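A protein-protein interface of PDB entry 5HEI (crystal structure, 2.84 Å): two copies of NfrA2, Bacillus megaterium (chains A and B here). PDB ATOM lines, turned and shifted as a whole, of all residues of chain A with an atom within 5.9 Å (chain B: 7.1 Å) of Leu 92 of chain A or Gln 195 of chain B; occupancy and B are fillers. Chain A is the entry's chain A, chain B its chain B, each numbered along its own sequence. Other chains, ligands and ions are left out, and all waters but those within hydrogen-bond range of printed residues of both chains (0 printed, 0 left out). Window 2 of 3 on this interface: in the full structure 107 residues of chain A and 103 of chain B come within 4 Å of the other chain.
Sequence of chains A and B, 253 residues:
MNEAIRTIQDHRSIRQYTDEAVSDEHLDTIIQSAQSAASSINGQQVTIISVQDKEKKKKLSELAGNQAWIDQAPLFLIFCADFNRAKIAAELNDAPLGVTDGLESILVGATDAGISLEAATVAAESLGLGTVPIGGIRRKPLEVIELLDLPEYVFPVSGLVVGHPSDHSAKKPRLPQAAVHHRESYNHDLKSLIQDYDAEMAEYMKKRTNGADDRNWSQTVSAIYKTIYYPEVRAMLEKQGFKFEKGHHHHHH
The side-chain hydroxyl of Ser 222 of chain B lies within hydrogen-bond range of the backbone carbonyl oxygen of Ala 89 of chain A, 3.0 Å away. The side-chain amide nitrogen of Asn 93 of chain A lies within hydrogen-bond range of the side-chain hydroxyl of Ser 218 of chain B. ND2 of Asn 93 of chain A is in hydrogen-bond range of OG of Ser 222 of chain B (3.0 Å).
Printed residues of chain B that touch a printed residue of chain A: Leu 190, Lys 191, Ile 194, Gln 195, Ser 218 and Ser 222. Among the printed residues, 11 pairs touch across the chains.
Among the printed residues, pairs that only touch across the chains: Ile 88 of chain A with Leu 190 of chain B (3.99 Å), Ile 88 of chain A with Lys 191 of chain B (3.9 Å), Ile 88 of chain A with Ile 194 of chain B (3.8 Å), Ala 89 of chain A with Ser 218 of chain B (3.9 Å), Ala 90 of chain A with Ser 222 of chain B (3.5 Å), Leu 92 of chain A with Lys 191 of chain B (3.999 Å), Leu 92 of chain A with Ile 194 of chain B (3.7 Å) and Leu 92 of chain A with Gln 195 of chain B (3.5 Å).
No position is printed for both chains. Of the 11 pairs that touch across the chains among the printed residues, none has its exchanged pair printed and touching as well.
Printed residues of chain B within 4 Å of Ile 88 of chain A: Leu 190 (3.99 Å), Lys 191 (3.9 Å) and Ile 194 (3.8 Å). Glu 91 of chain A touches none of the printed residues of chain B. Of the printed residues of chain B, Leu 92 of chain A touches Lys 191 (3.999 Å), Ile 194 (3.7 Å) and Gln 195 (3.5 Å). Of the printed residues of chain B, Asn 93 of chain A touches Ser 218 and Ser 222. Asp 94 of chain A touches none of the printed residues of chain B. Of the printed residues of chain A, Ile 194 of chain B touches Ile 88 and Leu 92. Gln 195 of chain B touches just one residue of chain A: Leu 92. Printed residues of chain A within 4 Å of Ser 222 of chain B: Ala 89 (3.0 Å), Ala 90 (3.5 Å) and Asn 93 (3.0 Å). The nearest printed residue of chain B that does not touch Leu 92 of chain A is Asp 198 of chain B (4.5 Å).
O of Ala 89 of chain A sits at hydrogen-bond distance from ND2 of Asn 93 of chain A (2.8 Å). The side-chain hydroxyl (OG) of Ser 222 of chain B sits at hydrogen-bond distance from the backbone carbonyl oxygen (O) of Ser 218 of chain B. N of Ser 218 of chain B sits at hydrogen-bond distance from OD1 of Asp 198 of chain B, at 2.8 Å.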
ATOM      1  N   LYS A  87      21.179  16.551  15.136  1.00  0.00           N
ATOM      2  CA  LYS A  87      20.289  16.405  16.291  1.00  0.00           C
ATOM      3  C   LYS A  87      20.698  15.166  17.098  1.00  0.00           C
ATOM      4  O   LYS A  87      20.763  15.258  18.324  1.00  0.00           O
ATOM      5  CB  LYS A  87      18.814  16.331  15.850  1.00  0.00           C
ATOM      6  CG  LYS A  87      17.805  16.477  16.988  1.00  0.00           C
ATOM      7  CD  LYS A  87      17.134  15.143  17.305  1.00  0.00           C
ATOM      8  CE  LYS A  87      16.060  15.244  18.354  1.00  0.00           C
ATOM      9  NZ  LYS A  87      15.402  13.929  18.572  1.00  0.00           N
ATOM     10  N   ILE A  88      20.994  14.023  16.420  1.00  0.00           N
ATOM     11  CA  ILE A  88      21.455  12.786  17.076  1.00  0.00           C
ATOM     12  C   ILE A  88      22.814  13.069  17.729  1.00  0.00           C
ATOM     13  O   ILE A  88      23.022  12.680  18.880  1.00  0.00           O
ATOM     14  CB  ILE A  88      21.515  11.545  16.123  1.00  0.00           C
ATOM     15  CG1 ILE A  88      20.160  11.263  15.441  1.00  0.00           C
ATOM     16  CG2 ILE A  88      22.008  10.292  16.872  1.00  0.00           C
ATOM     17  CD1 ILE A  88      20.245  10.493  14.124  1.00  0.00           C
ATOM     18  N   ALA A  89      23.714  13.775  16.999  1.00  0.00           N
ATOM     19  CA  ALA A  89      25.052  14.161  17.464  1.00  0.00           C
ATOM     20  C   ALA A  89      24.975  15.001  18.741  1.00  0.00           C
ATOM     21  O   ALA A  89      25.714  14.725  19.688  1.00  0.00           O
ATOM     22  CB  ALA A  89      25.793  14.922  16.372  1.00  0.00           C
ATOM     23  N   ALA A  90      24.055  15.994  18.777  1.00  0.00           N
ATOM     24  CA  ALA A  90      23.820  16.872  19.919  1.00  0.00           C
ATOM     25  C   ALA A  90      23.259  16.093  21.120  1.00  0.00           C
ATOM     26  O   ALA A  90      23.641  16.376  22.258  1.00  0.00           O
ATOM     27  CB  ALA A  90      22.881  17.996  19.524  1.00  0.00           C
ATOM     28  N   GLU A  91      22.382  15.093  20.859  1.00  0.00           N
ATOM     29  CA  GLU A  91      21.775  14.229  21.881  1.00  0.00           C
ATOM     30  C   GLU A  91      22.819  13.314  22.523  1.00  0.00           C
ATOM     31  O   GLU A  91      22.767  13.074  23.733  1.00  0.00           O
ATOM     32  CB  GLU A  91      20.631  13.393  21.289  1.00  0.00           C
ATOM     33  CG  GLU A  91      19.315  14.144  21.170  1.00  0.00           C
ATOM     34  CD  GLU A  91      18.149  13.337  20.626  1.00  0.00           C
ATOM     35  OE1 GLU A  91      18.260  12.806  19.496  1.00  0.00           O
ATOM     36  OE2 GLU A  91      17.104  13.275  21.313  1.00  0.00           O
ATOM     37  N   LEU A  92      23.773  12.819  21.708  1.00  0.00           N
ATOM     38  CA  LEU A  92      24.869  11.948  22.147  1.00  0.00           C
ATOM     39  C   LEU A  92      25.865  12.674  23.057  1.00  0.00           C
ATOM     40  O   LEU A  92      26.520  12.026  23.877  1.00  0.00           O
ATOM     41  CB  LEU A  92      25.607  11.347  20.934  1.00  0.00           C
ATOM     42  CG  LEU A  92      24.915  10.198  20.199  1.00  0.00           C
ATOM     43  CD1 LEU A  92      25.357  10.140  18.768  1.00  0.00           C
ATOM     44  CD2 LEU A  92      25.170   8.866  20.880  1.00  0.00           C
ATOM     45  N   ASN A  93      25.979  14.010  22.907  1.00  0.00           N
ATOM     46  CA  ASN A  93      26.899  14.850  23.674  1.00  0.00           C
ATOM     47  C   ASN A  93      26.202  15.791  24.671  1.00  0.00           C
ATOM     48  O   ASN A  93      26.837  16.736  25.158  1.00  0.00           O
ATOM     49  CB  ASN A  93      27.831  15.621  22.735  1.00  0.00           C
ATOM     50  CG  ASN A  93      28.697  14.723  21.895  1.00  0.00           C
ATOM     51  OD1 ASN A  93      29.663  14.115  22.366  1.00  0.00           O
ATOM     52  ND2 ASN A  93      28.344  14.595  20.639  1.00  0.00           N
ATOM     53  N   ASP A  94      24.910  15.511  24.993  1.00  0.00           N
ATOM     54  CA  ASP A  94      24.069  16.273  25.931  1.00  0.00           C
ATOM     55  C   ASP A  94      24.156  17.792  25.638  1.00  0.00           C
ATOM     56  O   ASP A  94      24.411  18.605  26.537  1.00  0.00           O
ATOM     57  CB  ASP A  94      24.450  15.924  27.396  1.00  0.00           C
ATOM     58  CG  ASP A  94      23.366  16.111  28.448  1.00  0.00           C
ATOM     59  OD1 ASP A  94      22.674  17.156  28.416  1.00  0.00           O
ATOM     60  OD2 ASP A  94      23.265  15.254  29.354  1.00  0.00           O
ATOM     61  N   LEU B 190      19.786   5.620  12.816  1.00  0.00           N
ATOM     62  CA  LEU B 190      21.112   6.162  12.480  1.00  0.00           C
ATOM     63  C   LEU B 190      22.036   6.386  13.684  1.00  0.00           C
ATOM     64  O   LEU B 190      23.224   6.653  13.485  1.00  0.00           O
ATOM     65  CB  LEU B 190      21.011   7.462  11.641  1.00  0.00           C
ATOM     66  CG  LEU B 190      20.099   7.488  10.415  1.00  0.00           C
ATOM     67  CD1 LEU B 190      20.027   8.874   9.821  1.00  0.00           C
ATOM     68  CD2 LEU B 190      20.551   6.497   9.360  1.00  0.00           C
ATOM     69  N   LYS B 191      21.504   6.279  14.918  1.00  0.00           N
ATOM     70  CA  LYS B 191      22.253   6.491  16.161  1.00  0.00           C
ATOM     71  C   LYS B 191      23.458   5.553  16.285  1.00  0.00           C
ATOM     72  O   LYS B 191      24.561   6.026  16.562  1.00  0.00           O
ATOM     73  CB  LYS B 191      21.317   6.373  17.379  1.00  0.00           C
ATOM     74  CG  LYS B 191      21.916   6.872  18.688  1.00  0.00           C
ATOM     75  CD  LYS B 191      20.873   6.875  19.799  1.00  0.00           C
ATOM     76  CE  LYS B 191      21.436   7.355  21.113  1.00  0.00           C
ATOM     77  NZ  LYS B 191      22.238   6.307  21.801  1.00  0.00           N
ATOM     78  N   SER B 192      23.251   4.238  16.054  1.00  0.00           N
ATOM     79  CA  SER B 192      24.291   3.210  16.120  1.00  0.00           C
ATOM     80  C   SER B 192      25.382   3.440  15.071  1.00  0.00           C
ATOM     81  O   SER B 192      26.558   3.234  15.367  1.00  0.00           O
ATOM     82  CB  SER B 192      23.682   1.821  15.961  1.00  0.00           C
ATOM     83  OG  SER B 192      22.800   1.527  17.034  1.00  0.00           O
ATOM     84  N   LEU B 193      24.985   3.893  13.862  1.00  0.00           N
ATOM     85  CA  LEU B 193      25.885   4.203  12.748  1.00  0.00           C
ATOM     86  C   LEU B 193      26.765   5.413  13.060  1.00  0.00           C
ATOM     87  O   LEU B 193      27.929   5.425  12.669  1.00  0.00           O
ATOM     88  CB  LEU B 193      25.086   4.456  11.460  1.00  0.00           C
ATOM     89  CG  LEU B 193      24.687   3.222  10.670  1.00  0.00           C
ATOM     90  CD1 LEU B 193      23.225   2.903  10.857  1.00  0.00           C
ATOM     91  CD2 LEU B 193      24.955   3.425   9.212  1.00  0.00           C
ATOM     92  N   ILE B 194      26.209   6.425  13.758  1.00  0.00           N
ATOM     93  CA  ILE B 194      26.932   7.636  14.160  1.00  0.00           C
ATOM     94  C   ILE B 194      27.944   7.266  15.253  1.00  0.00           C
ATOM     95  O   ILE B 194      29.092   7.709  15.191  1.00  0.00           O
ATOM     96  CB  ILE B 194      25.960   8.793  14.558  1.00  0.00           C
ATOM     97  CG1 ILE B 194      25.242   9.336  13.308  1.00  0.00           C
ATOM     98  CG2 ILE B 194      26.689   9.926  15.300  1.00  0.00           C
ATOM     99  CD1 ILE B 194      23.925  10.017  13.554  1.00  0.00           C
ATOM    100  N   GLN B 195      27.519   6.421  16.220  1.00  0.00           N
ATOM    101  CA  GLN B 195      28.349   5.933  17.328  1.00  0.00           C
ATOM    102  C   GLN B 195      29.584   5.168  16.822  1.00  0.00           C
ATOM    103  O   GLN B 195      30.687   5.380  17.334  1.00  0.00           O
ATOM    104  CB  GLN B 195      27.516   5.077  18.297  1.00  0.00           C
ATOM    105  CG  GLN B 195      26.627   5.903  19.225  1.00  0.00           C
ATOM    106  CD  GLN B 195      25.706   5.073  20.092  1.00  0.00           C
ATOM    107  OE1 GLN B 195      25.036   4.138  19.631  1.00  0.00           O
ATOM    108  NE2 GLN B 195      25.604   5.442  21.364  1.00  0.00           N
ATOM    109  N   ASP B 196      29.399   4.316  15.788  1.00  0.00           N
ATOM    110  CA  ASP B 196      30.483   3.548  15.165  1.00  0.00           C
ATOM    111  C   ASP B 196      31.395   4.476  14.358  1.00  0.00           C
ATOM    112  O   ASP B 196      32.604   4.256  14.300  1.00  0.00           O
ATOM    113  CB  ASP B 196      29.919   2.437  14.265  1.00  0.00           C
ATOM    114  CG  ASP B 196      29.141   1.356  14.995  1.00  0.00           C
ATOM    115  OD1 ASP B 196      29.536   0.994  16.129  1.00  0.00           O
ATOM    116  OD2 ASP B 196      28.168   0.833  14.412  1.00  0.00           O
ATOM    117  N   TYR B 197      30.792   5.525  13.755  1.00  0.00           N
ATOM    118  CA  TYR B 197      31.461   6.556  12.964  1.00  0.00           C
ATOM    119  C   TYR B 197      32.351   7.444  13.846  1.00  0.00           C
ATOM    120  O   TYR B 197      33.405   7.879  13.392  1.00  0.00           O
ATOM    121  CB  TYR B 197      30.425   7.386  12.177  1.00  0.00           C
ATOM    122  CG  TYR B 197      31.016   8.472  11.306  1.00  0.00           C
ATOM    123  CD1 TYR B 197      31.932   8.169  10.303  1.00  0.00           C
ATOM    124  CD2 TYR B 197      30.634   9.801  11.460  1.00  0.00           C
ATOM    125  CE1 TYR B 197      32.493   9.168   9.511  1.00  0.00           C
ATOM    126  CE2 TYR B 197      31.165  10.805  10.652  1.00  0.00           C
ATOM    127  CZ  TYR B 197      32.092  10.484   9.674  1.00  0.00           C
ATOM    128  OH  TYR B 197      32.627  11.476   8.888  1.00  0.00           O
ATOM    129  N   ASP B 198      31.927   7.692  15.100  1.00  0.00           N
ATOM    130  CA  ASP B 198      32.645   8.478  16.101  1.00  0.00           C
ATOM    131  C   ASP B 198      33.902   7.740  16.546  1.00  0.00           C
ATOM    132  O   ASP B 198      34.925   8.383  16.800  1.00  0.00           O
ATOM    133  CB  ASP B 198      31.742   8.755  17.320  1.00  0.00           C
ATOM    134  CG  ASP B 198      30.816   9.951  17.200  1.00  0.00           C
ATOM    135  OD1 ASP B 198      31.199  10.936  16.527  1.00  0.00           O
ATOM    136  OD2 ASP B 198      29.745   9.935  17.838  1.00  0.00           O
ATOM    137  N   ALA B 199      33.822   6.390  16.647  1.00  0.00           N
ATOM    138  CA  ALA B 199      34.929   5.518  17.038  1.00  0.00           C
ATOM    139  C   ALA B 199      36.010   5.524  15.952  1.00  0.00           C
ATOM    140  O   ALA B 199      37.202   5.537  16.278  1.00  0.00           O
ATOM    141  CB  ALA B 199      34.423   4.105  17.278  1.00  0.00           C
ATOM    142  N   GLU B 200      35.589   5.557  14.669  1.00  0.00           N
ATOM    143  CA  GLU B 200      36.462   5.588  13.494  1.00  0.00           C
ATOM    144  C   GLU B 200      37.018   7.003  13.255  1.00  0.00           C
ATOM    145  O   GLU B 200      38.053   7.149  12.602  1.00  0.00           O
ATOM    146  CB  GLU B 200      35.707   5.066  12.255  1.00  0.00           C
ATOM    147  CG  GLU B 200      36.589   4.366  11.230  1.00  0.00           C
ATOM    148  CD  GLU B 200      36.403   2.862  11.117  1.00  0.00           C
ATOM    149  OE1 GLU B 200      37.119   2.116  11.826  1.00  0.00           O
ATOM    150  OE2 GLU B 200      35.565   2.429  10.294  1.00  0.00           O
ATOM    151  N   TRP B 217      33.474  12.885  15.619  1.00  0.00           N
ATOM    152  CA  TRP B 217      32.610  13.656  14.727  1.00  0.00           C
ATOM    153  C   TRP B 217      31.490  14.406  15.464  1.00  0.00           C
ATOM    154  O   TRP B 217      31.322  15.606  15.245  1.00  0.00           O
ATOM    155  CB  TRP B 217      32.048  12.752  13.621  1.00  0.00           C
ATOM    156  CG  TRP B 217      31.095  13.438  12.690  1.00  0.00           C
ATOM    157  CD1 TRP B 217      31.414  14.205  11.608  1.00  0.00           C
ATOM    158  CD2 TRP B 217      29.666  13.356  12.716  1.00  0.00           C
ATOM    159  NE1 TRP B 217      30.269  14.624  10.970  1.00  0.00           N
ATOM    160  CE2 TRP B 217      29.181  14.118  11.630  1.00  0.00           C
ATOM    161  CE3 TRP B 217      28.741  12.716  13.561  1.00  0.00           C
ATOM    162  CZ2 TRP B 217      27.815  14.264  11.369  1.00  0.00           C
ATOM    163  CZ3 TRP B 217      27.389  12.864  13.303  1.00  0.00           C
ATOM    164  CH2 TRP B 217      26.937  13.633  12.220  1.00  0.00           C
ATOM    165  N   SER B 218      30.733  13.696  16.320  1.00  0.00           N
ATOM    166  CA  SER B 218      29.605  14.246  17.064  1.00  0.00           C
ATOM    167  C   SER B 218      29.988  15.409  17.961  1.00  0.00           C
ATOM    168  O   SER B 218      29.239  16.380  18.017  1.00  0.00           O
ATOM    169  CB  SER B 218      28.890  13.155  17.852  1.00  0.00           C
ATOM    170  OG  SER B 218      29.623  12.766  19.001  1.00  0.00           O
ATOM    171  N   SER B 222      28.359  19.020  17.536  1.00  0.00           N
ATOM    172  CA  SER B 222      27.557  19.495  18.680  1.00  0.00           C
ATOM    173  C   SER B 222      27.929  20.913  19.084  1.00  0.00           C
ATOM    174  O   SER B 222      27.052  21.765  19.160  1.00  0.00           O
ATOM    175  CB  SER B 222      27.725  18.578  19.890  1.00  0.00           C
ATOM    176  OG  SER B 222      27.286  17.254  19.641  1.00  0.00           O
